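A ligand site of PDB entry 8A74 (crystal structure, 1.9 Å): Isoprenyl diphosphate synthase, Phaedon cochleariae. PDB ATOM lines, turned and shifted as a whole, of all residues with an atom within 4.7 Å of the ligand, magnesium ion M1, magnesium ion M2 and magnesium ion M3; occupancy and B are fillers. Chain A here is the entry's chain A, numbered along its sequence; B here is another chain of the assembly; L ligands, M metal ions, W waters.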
ATOM      1  N   GLN A  89      24.958  11.423   2.034  1.00  0.00           N
ATOM      2  CA  GLN A  89      23.527  11.764   2.244  1.00  0.00           C
ATOM      3  C   GLN A  89      22.680  11.087   1.167  1.00  0.00           C
ATOM      4  O   GLN A  89      21.726  10.362   1.521  1.00  0.00           O
ATOM      5  CB  GLN A  89      23.361  13.290   2.231  1.00  0.00           C
ATOM      6  CG  GLN A  89      21.911  13.768   2.253  1.00  0.00           C
ATOM      7  CD  GLN A  89      21.242  13.507   3.579  1.00  0.00           C
ATOM      8  OE1 GLN A  89      20.938  14.432   4.323  1.00  0.00           O
ATOM      9  NE2 GLN A  89      21.021  12.242   3.882  1.00  0.00           N
ATOM     10  N   LEU A  92      22.399   7.259   1.491  1.00  0.00           N
ATOM     11  CA  LEU A  92      21.548   6.885   2.654  1.00  0.00           C
ATOM     12  C   LEU A  92      20.074   7.012   2.279  1.00  0.00           C
ATOM     13  O   LEU A  92      19.300   6.073   2.568  1.00  0.00           O
ATOM     14  CB  LEU A  92      21.895   7.771   3.863  1.00  0.00           C
ATOM     15  CG  LEU A  92      23.278   7.579   4.457  1.00  0.00           C
ATOM     16  CD1 LEU A  92      23.536   8.613   5.551  1.00  0.00           C
ATOM     17  CD2 LEU A  92      23.468   6.178   5.015  1.00  0.00           C
ATOM     18  N   LEU A  93      19.691   8.128   1.660  1.00  0.00           N
ATOM     19  CA  LEU A  93      18.281   8.450   1.319  1.00  0.00           C
ATOM     20  C   LEU A  93      17.777   7.509   0.220  1.00  0.00           C
ATOM     21  O   LEU A  93      16.616   7.080   0.308  1.00  0.00           O
ATOM     22  CB  LEU A  93      18.178   9.932   0.912  1.00  0.00           C
ATOM     23  CG  LEU A  93      18.593  10.925   1.996  1.00  0.00           C
ATOM     24  CD1 LEU A  93      18.187  12.346   1.620  1.00  0.00           C
ATOM     25  CD2 LEU A  93      18.014  10.546   3.352  1.00  0.00           C
ATOM     26  N   MET A  95      18.719   4.381  -0.166  1.00  0.00           N
ATOM     27  CA  MET A  95      18.498   3.092   0.541  1.00  0.00           C
ATOM     28  C   MET A  95      17.270   3.197   1.437  1.00  0.00           C
ATOM     29  O   MET A  95      16.382   2.325   1.342  1.00  0.00           O
ATOM     30  CB  MET A  95      19.707   2.704   1.404  1.00  0.00           C
ATOM     31  CG  MET A  95      19.494   1.421   2.174  1.00  0.00           C
ATOM     32  SD  MET A  95      21.048   0.645   2.693  1.00  0.00           S
ATOM     33  CE  MET A  95      21.503  -0.200   1.176  1.00  0.00           C
ATOM     34  N   ASP A  96      17.221   4.231   2.289  1.00  0.00           N
ATOM     35  CA  ASP A  96      16.170   4.384   3.329  1.00  0.00           C
ATOM     36  C   ASP A  96      14.791   4.378   2.666  1.00  0.00           C
ATOM     37  O   ASP A  96      13.853   3.779   3.254  1.00  0.00           O
ATOM     38  CB  ASP A  96      16.388   5.655   4.150  1.00  0.00           C
ATOM     39  CG  ASP A  96      15.266   5.886   5.137  1.00  0.00           C
ATOM     40  OD1 ASP A  96      14.357   6.670   4.809  1.00  0.00           O
ATOM     41  OD2 ASP A  96      15.280   5.251   6.223  1.00  0.00           O
ATOM     42  N   ASP A  97      14.666   5.026   1.499  1.00  0.00           N
ATOM     43  CA  ASP A  97      13.393   5.131   0.742  1.00  0.00           C
ATOM     44  C   ASP A  97      12.946   3.736   0.294  1.00  0.00           C
ATOM     45  O   ASP A  97      11.752   3.424   0.481  1.00  0.00           O
ATOM     46  CB  ASP A  97      13.528   6.129  -0.412  1.00  0.00           C
ATOM     47  CG  ASP A  97      13.476   7.580   0.042  1.00  0.00           C
ATOM     48  OD1 ASP A  97      12.735   7.880   0.995  1.00  0.00           O
ATOM     49  OD2 ASP A  97      14.185   8.420  -0.557  1.00  0.00           O
ATOM     50  N   MET A  99      13.813   0.915   1.740  1.00  0.00           N
ATOM     51  CA  MET A  99      13.545   0.193   3.009  1.00  0.00           C
ATOM     52  C   MET A  99      12.166   0.586   3.559  1.00  0.00           C
ATOM     53  O   MET A  99      11.435  -0.329   4.023  1.00  0.00           O
ATOM     54  CB  MET A  99      14.639   0.499   4.047  1.00  0.00           C
ATOM     55  CG  MET A  99      15.940  -0.247   3.757  1.00  0.00           C
ATOM     56  SD  MET A  99      17.297   0.071   4.922  1.00  0.00           S
ATOM     57  CE  MET A  99      16.526  -0.375   6.482  1.00  0.00           C
ATOM     58  N   ASP A 100      11.795   1.865   3.480  1.00  0.00           N
ATOM     59  CA  ASP A 100      10.507   2.395   3.993  1.00  0.00           C
ATOM     60  C   ASP A 100       9.431   2.392   2.899  1.00  0.00           C
ATOM     61  O   ASP A 100       8.257   2.681   3.229  1.00  0.00           O
ATOM     62  CB  ASP A 100      10.668   3.806   4.565  1.00  0.00           C
ATOM     63  CG  ASP A 100      11.625   3.877   5.748  1.00  0.00           C
ATOM     64  OD1 ASP A 100      12.130   4.987   6.012  1.00  0.00           O
ATOM     65  OD2 ASP A 100      11.846   2.825   6.386  1.00  0.00           O
ATOM     66  N   SER A 102       8.873   4.491   0.605  1.00  0.00           N
ATOM     67  CA  SER A 102       8.324   5.868   0.527  1.00  0.00           C
ATOM     68  C   SER A 102       8.041   6.215  -0.939  1.00  0.00           C
ATOM     69  O   SER A 102       8.754   5.704  -1.823  1.00  0.00           O
ATOM     70  CB  SER A 102       9.257   6.867   1.172  1.00  0.00           C
ATOM     71  OG  SER A 102       9.334   6.647   2.568  1.00  0.00           O
ATOM     72  N   ARG A 105      10.543  11.880  -1.867  1.00  0.00           N
ATOM     73  CA  ARG A 105      11.405  12.619  -0.924  1.00  0.00           C
ATOM     74  C   ARG A 105      11.707  14.003  -1.503  1.00  0.00           C
ATOM     75  O   ARG A 105      12.233  14.059  -2.635  1.00  0.00           O
ATOM     76  CB  ARG A 105      12.720  11.890  -0.653  1.00  0.00           C
ATOM     77  CG  ARG A 105      13.603  12.638   0.335  1.00  0.00           C
ATOM     78  CD  ARG A 105      14.895  11.915   0.641  1.00  0.00           C
ATOM     79  NE  ARG A 105      14.675  10.642   1.306  1.00  0.00           N
ATOM     80  CZ  ARG A 105      14.390  10.486   2.597  1.00  0.00           C
ATOM     81  NH1 ARG A 105      14.256  11.542   3.396  1.00  0.00           N
ATOM     82  NH2 ARG A 105      14.223   9.279   3.095  1.00  0.00           N
ATOM     83  N   THR A 160      26.222   5.129  11.229  1.00  0.00           N
ATOM     84  CA  THR A 160      24.913   5.404  10.607  1.00  0.00           C
ATOM     85  C   THR A 160      24.152   4.090  10.396  1.00  0.00           C
ATOM     86  O   THR A 160      22.948   4.051  10.687  1.00  0.00           O
ATOM     87  CB  THR A 160      25.078   6.241   9.326  1.00  0.00           C
ATOM     88  OG1 THR A 160      25.827   7.412   9.666  1.00  0.00           O
ATOM     89  CG2 THR A 160      23.740   6.647   8.740  1.00  0.00           C
ATOM     90  N   ASN A 161      24.843   3.035   9.942  1.00  0.00           N
ATOM     91  CA  ASN A 161      24.228   1.697   9.728  1.00  0.00           C
ATOM     92  C   ASN A 161      23.725   1.124  11.063  1.00  0.00           C
ATOM     93  O   ASN A 161      22.622   0.548  11.072  1.00  0.00           O
ATOM     94  CB  ASN A 161      25.177   0.745   9.002  1.00  0.00           C
ATOM     95  CG  ASN A 161      25.171   0.998   7.508  1.00  0.00           C
ATOM     96  OD1 ASN A 161      26.141   1.529   6.963  1.00  0.00           O
ATOM     97  ND2 ASN A 161      24.081   0.653   6.845  1.00  0.00           N
ATOM     98  N   GLN A 164      20.473   2.944  11.739  1.00  0.00           N
ATOM     99  CA  GLN A 164      19.369   2.465  10.854  1.00  0.00           C
ATOM    100  C   GLN A 164      18.882   1.100  11.355  1.00  0.00           C
ATOM    101  O   GLN A 164      17.655   0.885  11.362  1.00  0.00           O
ATOM    102  CB  GLN A 164      19.837   2.398   9.395  1.00  0.00           C
ATOM    103  CG  GLN A 164      18.752   1.958   8.419  1.00  0.00           C
ATOM    104  CD  GLN A 164      17.795   3.054   8.040  1.00  0.00           C
ATOM    105  OE1 GLN A 164      17.579   4.015   8.773  1.00  0.00           O
ATOM    106  NE2 GLN A 164      17.216   2.929   6.861  1.00  0.00           N
ATOM    107  N   ASP A 167      16.827   1.589  14.601  1.00  0.00           N
ATOM    108  CA  ASP A 167      15.515   2.106  14.139  1.00  0.00           C
ATOM    109  C   ASP A 167      14.646   0.915  13.687  1.00  0.00           C
ATOM    110  O   ASP A 167      13.479   0.851  14.102  1.00  0.00           O
ATOM    111  CB  ASP A 167      15.699   3.141  13.036  1.00  0.00           C
ATOM    112  CG  ASP A 167      14.563   4.145  12.928  1.00  0.00           C
ATOM    113  OD1 ASP A 167      13.962   4.459  13.966  1.00  0.00           O
ATOM    114  OD2 ASP A 167      14.317   4.605  11.805  1.00  0.00           O
ATOM    115  N   LYS A 193      21.972   7.358  13.820  1.00  0.00           N
ATOM    116  CA  LYS A 193      21.301   7.359  12.486  1.00  0.00           C
ATOM    117  C   LYS A 193      21.462   8.721  11.790  1.00  0.00           C
ATOM    118  O   LYS A 193      21.522   8.723  10.545  1.00  0.00           O
ATOM    119  CB  LYS A 193      19.821   6.990  12.615  1.00  0.00           C
ATOM    120  CG  LYS A 193      19.140   6.629  11.301  1.00  0.00           C
ATOM    121  CD  LYS A 193      17.627   6.524  11.385  1.00  0.00           C
ATOM    122  CE  LYS A 193      16.957   7.874  11.453  1.00  0.00           C
ATOM    123  NZ  LYS A 193      15.476   7.746  11.392  1.00  0.00           N
ATOM    124  N   TYR A 197      26.340  11.929  10.988  1.00  0.00           N
ATOM    125  CA  TYR A 197      26.576  12.324   9.577  1.00  0.00           C
ATOM    126  C   TYR A 197      26.063  13.743   9.319  1.00  0.00           C
ATOM    127  O   TYR A 197      26.637  14.414   8.439  1.00  0.00           O
ATOM    128  CB  TYR A 197      25.997  11.285   8.610  1.00  0.00           C
ATOM    129  CG  TYR A 197      24.618  11.571   8.062  1.00  0.00           C
ATOM    130  CD1 TYR A 197      24.447  12.312   6.900  1.00  0.00           C
ATOM    131  CD2 TYR A 197      23.488  11.066   8.669  1.00  0.00           C
ATOM    132  CE1 TYR A 197      23.190  12.566   6.374  1.00  0.00           C
ATOM    133  CE2 TYR A 197      22.222  11.308   8.163  1.00  0.00           C
ATOM    134  CZ  TYR A 197      22.071  12.051   7.015  1.00  0.00           C
ATOM    135  OH  TYR A 197      20.820  12.281   6.524  1.00  0.00           O
ATOM    136  N   THR A 253       3.929  12.098   7.746  1.00  0.00           N
ATOM    137  CA  THR A 253       3.445  10.697   7.661  1.00  0.00           C
ATOM    138  C   THR A 253       4.153   9.818   8.708  1.00  0.00           C
ATOM    139  O   THR A 253       4.087   8.586   8.573  1.00  0.00           O
ATOM    140  CB  THR A 253       3.637  10.154   6.236  1.00  0.00           C
ATOM    141  OG1 THR A 253       5.017  10.294   5.889  1.00  0.00           O
ATOM    142  CG2 THR A 253       2.771  10.855   5.212  1.00  0.00           C
ATOM    143  N   GLU A 257       3.514   5.840   9.241  1.00  0.00           N
ATOM    144  CA  GLU A 257       4.739   5.019   9.020  1.00  0.00           C
ATOM    145  C   GLU A 257       5.152   4.289  10.304  1.00  0.00           C
ATOM    146  O   GLU A 257       6.025   3.398  10.206  1.00  0.00           O
ATOM    147  CB  GLU A 257       5.867   5.897   8.472  1.00  0.00           C
ATOM    148  CG  GLU A 257       5.676   6.285   7.016  1.00  0.00           C
ATOM    149  CD  GLU A 257       6.656   7.318   6.494  1.00  0.00           C
ATOM    150  OE1 GLU A 257       7.356   7.022   5.500  1.00  0.00           O
ATOM    151  OE2 GLU A 257       6.723   8.410   7.083  1.00  0.00           O
ATOM    152  N   LYS A 259       6.804   5.447  12.998  1.00  0.00           N
ATOM    153  CA  LYS A 259       8.218   5.788  13.319  1.00  0.00           C
ATOM    154  C   LYS A 259       8.393   5.915  14.831  1.00  0.00           C
ATOM    155  O   LYS A 259       7.410   6.293  15.522  1.00  0.00           O
ATOM    156  CB  LYS A 259       8.641   7.090  12.630  1.00  0.00           C
ATOM    157  CG  LYS A 259       8.915   6.978  11.147  1.00  0.00           C
ATOM    158  CD  LYS A 259       9.661   8.167  10.608  1.00  0.00           C
ATOM    159  CE  LYS A 259       9.589   8.298   9.105  1.00  0.00           C
ATOM    160  NZ  LYS A 259       9.870   9.687   8.665  1.00  0.00           N
ATOM    161  N   ASN B 123      20.158  -2.635   4.596  1.00  0.00           N
ATOM    162  CA  ASN B 123      21.356  -1.836   4.959  1.00  0.00           C
ATOM    163  C   ASN B 123      22.448  -2.741   5.556  1.00  0.00           C
ATOM    164  O   ASN B 123      23.548  -2.216   5.818  1.00  0.00           O
ATOM    165  CB  ASN B 123      21.012  -0.682   5.905  1.00  0.00           C
ATOM    166  CG  ASN B 123      20.716  -1.134   7.316  1.00  0.00           C
ATOM    167  OD1 ASN B 123      19.710  -1.795   7.561  1.00  0.00           O
ATOM    168  ND2 ASN B 123      21.578  -0.768   8.262  1.00  0.00           N
ATOM    169  N   LEU B 126      25.450  -2.725   3.185  1.00  0.00           N
ATOM    170  CA  LEU B 126      26.230  -1.467   3.352  1.00  0.00           C
ATOM    171  C   LEU B 126      27.072  -1.556   4.641  1.00  0.00           C
ATOM    172  O   LEU B 126      28.252  -1.139   4.610  1.00  0.00           O
ATOM    173  CB  LEU B 126      25.276  -0.270   3.401  1.00  0.00           C
ATOM    174  CG  LEU B 126      25.949   1.104   3.462  1.00  0.00           C
ATOM    175  CD1 LEU B 126      26.744   1.390   2.197  1.00  0.00           C
ATOM    176  CD2 LEU B 126      24.914   2.197   3.683  1.00  0.00           C
HETATM  177  C1  LIG L   1      15.833   8.758   7.174  1.00  0.00           C
HETATM  178  O1  LIG L   1      15.173   8.496   8.409  1.00  0.00           O
HETATM  179  C2  LIG L   1      17.095   7.935   7.127  1.00  0.00           C
HETATM  180  C3  LIG L   1      18.354   8.346   7.250  1.00  0.00           C
HETATM  181  C4  LIG L   1      18.800   9.772   7.107  1.00  0.00           C
HETATM  182  C5  LIG L   1      19.470   7.376   7.578  1.00  0.00           C
HETATM  183  C6  LIG L   1      19.390   6.055   6.815  1.00  0.00           C
HETATM  184  C7  LIG L   1      20.547   5.155   7.087  1.00  0.00           C
HETATM  185  C8  LIG L   1      20.960   4.093   6.399  1.00  0.00           C
HETATM  186  C9  LIG L   1      20.298   3.624   5.138  1.00  0.00           C
HETATM  187  C10 LIG L   1      22.136   3.269   6.816  1.00  0.00           C
HETATM  188  P1  LIG L   1      13.589   8.169   8.458  1.00  0.00           P
HETATM  189  O2  LIG L   1      13.271   7.040   7.530  1.00  0.00           O
HETATM  190  O3  LIG L   1      13.191   8.035   9.885  1.00  0.00           O
HETATM  191  O4  LIG L   1      12.945   9.535   7.903  1.00  0.00           O
HETATM  192  P2  LIG L   1      12.552  10.114   6.457  1.00  0.00           P
HETATM  193  O5  LIG L   1      12.752   8.998   5.462  1.00  0.00           O
HETATM  194  O6  LIG L   1      13.496  11.280   6.227  1.00  0.00           O
HETATM  195  O7  LIG L   1      11.100  10.542   6.574  1.00  0.00           O
HETATM  196 MG    MG M   1      12.387   6.901   5.522  1.00  0.00          MG
HETATM  197 MG    MG M   2      13.720   4.834   7.656  1.00  0.00          MG
HETATM  198 MG    MG M   3       9.427  11.088   5.256  1.00  0.00          MG
HETATM  199  O   HOH W   1      12.158   4.586   9.007  1.00  0.00           O
HETATM  200  O   HOH W   2      10.405   7.107   6.089  1.00  0.00           O
HETATM  201  O   HOH W   3      12.030  10.232  11.121  1.00  0.00           O
HETATM  202  O   HOH W   4      11.806   6.822   3.545  1.00  0.00           O
HETATM  203  O   HOH W   5      12.742  13.711   6.218  1.00  0.00           O
HETATM  204  O   HOH W   6       9.098   8.888   4.599  1.00  0.00           O
HETATM  205  O   HOH W   7       8.126  10.815   6.735  1.00  0.00           O
HETATM  206  O   HOH W   8      15.190   5.152   9.139  1.00  0.00           O
HETATM  207  O   HOH W   9       8.190  11.893   3.999  1.00  0.00           O
HETATM  208  O   HOH W  10      10.871  11.535   3.606  1.00  0.00           O
HETATM  209  O   HOH W  11       9.809  13.047   6.075  1.00  0.00           O
HETATM  210  O   HOH W  12      14.253   2.943   7.721  1.00  0.00           O
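An oxygen (O3) of the ligand lies within salt-bridge range of the side-chain amino group of Lys 259 (3.9 Å). NZ of Lys 193 is in salt-bridge range of O3 of the ligand, 2.8 Å away. O6 of the ligand lies within salt-bridge range of NH1 of Arg 105, 2.9 Å away.
OD1 of Asp 96 lies close to NH2 of Arg 105. The side-chain carboxylate (OD2) of Asp 96 lies close to the side-chain amide nitrogen (NE2) of Gln 164 (3.1 Å). The side-chain amino group of Lys 259 lies within salt-bridge range of the side-chain carboxylate of Glu 257 (3.7 Å). The side-chain amino group of Lys 193 lies within salt-bridge range of the side-chain carboxylate of Asp 167, 3.4 Å away. The guanidinium group of Arg 105 lies within salt-bridge range of the side-chain carboxylate of Asp 97, at 2.9 Å. The backbone carbonyl oxygen (O) of Asn 123 of chain B lies within hydrogen-bond range of the side-chain amide nitrogen (ND2) of Asn 161, 3.1 Å away. The side-chain amide nitrogen (NE2) of Gln 89 lies within hydrogen-bond range of the side-chain hydroxyl (OH) of Tyr 197 (2.6 Å). The side-chain amide nitrogen (NE2) of Gln 164 sits close to the side-chain sulfur (SD) of Met 99, at 3.5 Å.
Leu 92 touches the ligand. CD2 of Leu 93 touches C4 of the ligand (3.9 Å). Met 95 touches the ligand. Thr 160 touches the ligand. Asn 161 touches the ligand. Gln 164 touches the ligand. Tyr 197 touches the ligand (OH to C4, 3.3 Å). Hydrophobic or aromatic side chains that line the ligand: Leu 92, Leu 93, Met 95 and Tyr 197. 12 residues have an atom within 4 Å of the ligand: Leu 92, Leu 93, Met 95, Asp 96, Asp 100, Arg 105, Thr 160, Asn 161, Gln 164, Lys 193, Tyr 197 and Lys 259.
Merely in contact with magnesium ion M1: Arg 105 (3.9 Å). Of the 21 residues printed, 3 come within 4 Å of magnesium ion M1. Along chain A the residues within 4 Å of magnesium ion M1 span positions 96 to 105. The nearest printed residue that does not touch magnesium ion M1 is Ser 102 (4.3 Å).
Two residues have an atom within 4 Å of magnesium ion M2: Asp 96 and Asp 100.
Lys 259 touches magnesium ion M3 (NZ to MG, 3.7 Å). Of the 21 residues printed, 1 comes within 4 Å of magnesium ion M3. The nearest printed residue that does not touch magnesium ion M3 is Glu 257 (4.2 Å).
Magnesium ion M1 is bound by OD1 of Asp 100 (2.0 Å), water W4 (2.1 Å), water W2 (2.1 Å), OD1 of Asp 96 (2.1 Å), O5 of the ligand (2.1 Å) and O2 of the ligand (2.2 Å).
Water W12 binds magnesium ion M2. Water W1 binds magnesium ion M2 (2.1 Å). Water W8 is bound to magnesium ion M2. Magnesium ion M2 is bound by the side-chain carboxylate (OD2) of Asp 96 (2.2 Å). O2 of the ligand binds magnesium ion M2 (2.3 Å). The side-chain carboxylate (OD1) of Asp 100 binds magnesium ion M2. Magnesium ion M2 has six donor atoms within binding distance.
Magnesium ion M3 is bound by water W9 (1.9 Å), water W7 (2.0 Å), water W11 (2.2 Å), an oxygen (O7) of the ligand (2.2 Å), water W10 (2.2 Å) and water W6 (2.3 Å).
Water W4 lies within hydrogen-bond range of OG of Ser 102 (2.7 Å), OD1 of Asp 97 (2.9 Å) and NH2 of Arg 105 (3.5 Å). Water W12 bridges OD2 of Asp 100 (2.8 Å) and NE2 of Gln 164 (3.1 Å). Water W7 lies within hydrogen-bond range of OE2 of Glu 257 (2.8 Å), NZ of Lys 259 (2.8 Å) and OG1 of Thr 253 (3.3 Å). Water W6 bridges the side-chain carboxylate of Glu 257 and the side-chain hydroxyl of Ser 102. Water W3 bridges an oxygen (O3) of the ligand (2.8 Å) and the side-chain amino group (NZ) of Lys 259 (3.3 Å).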
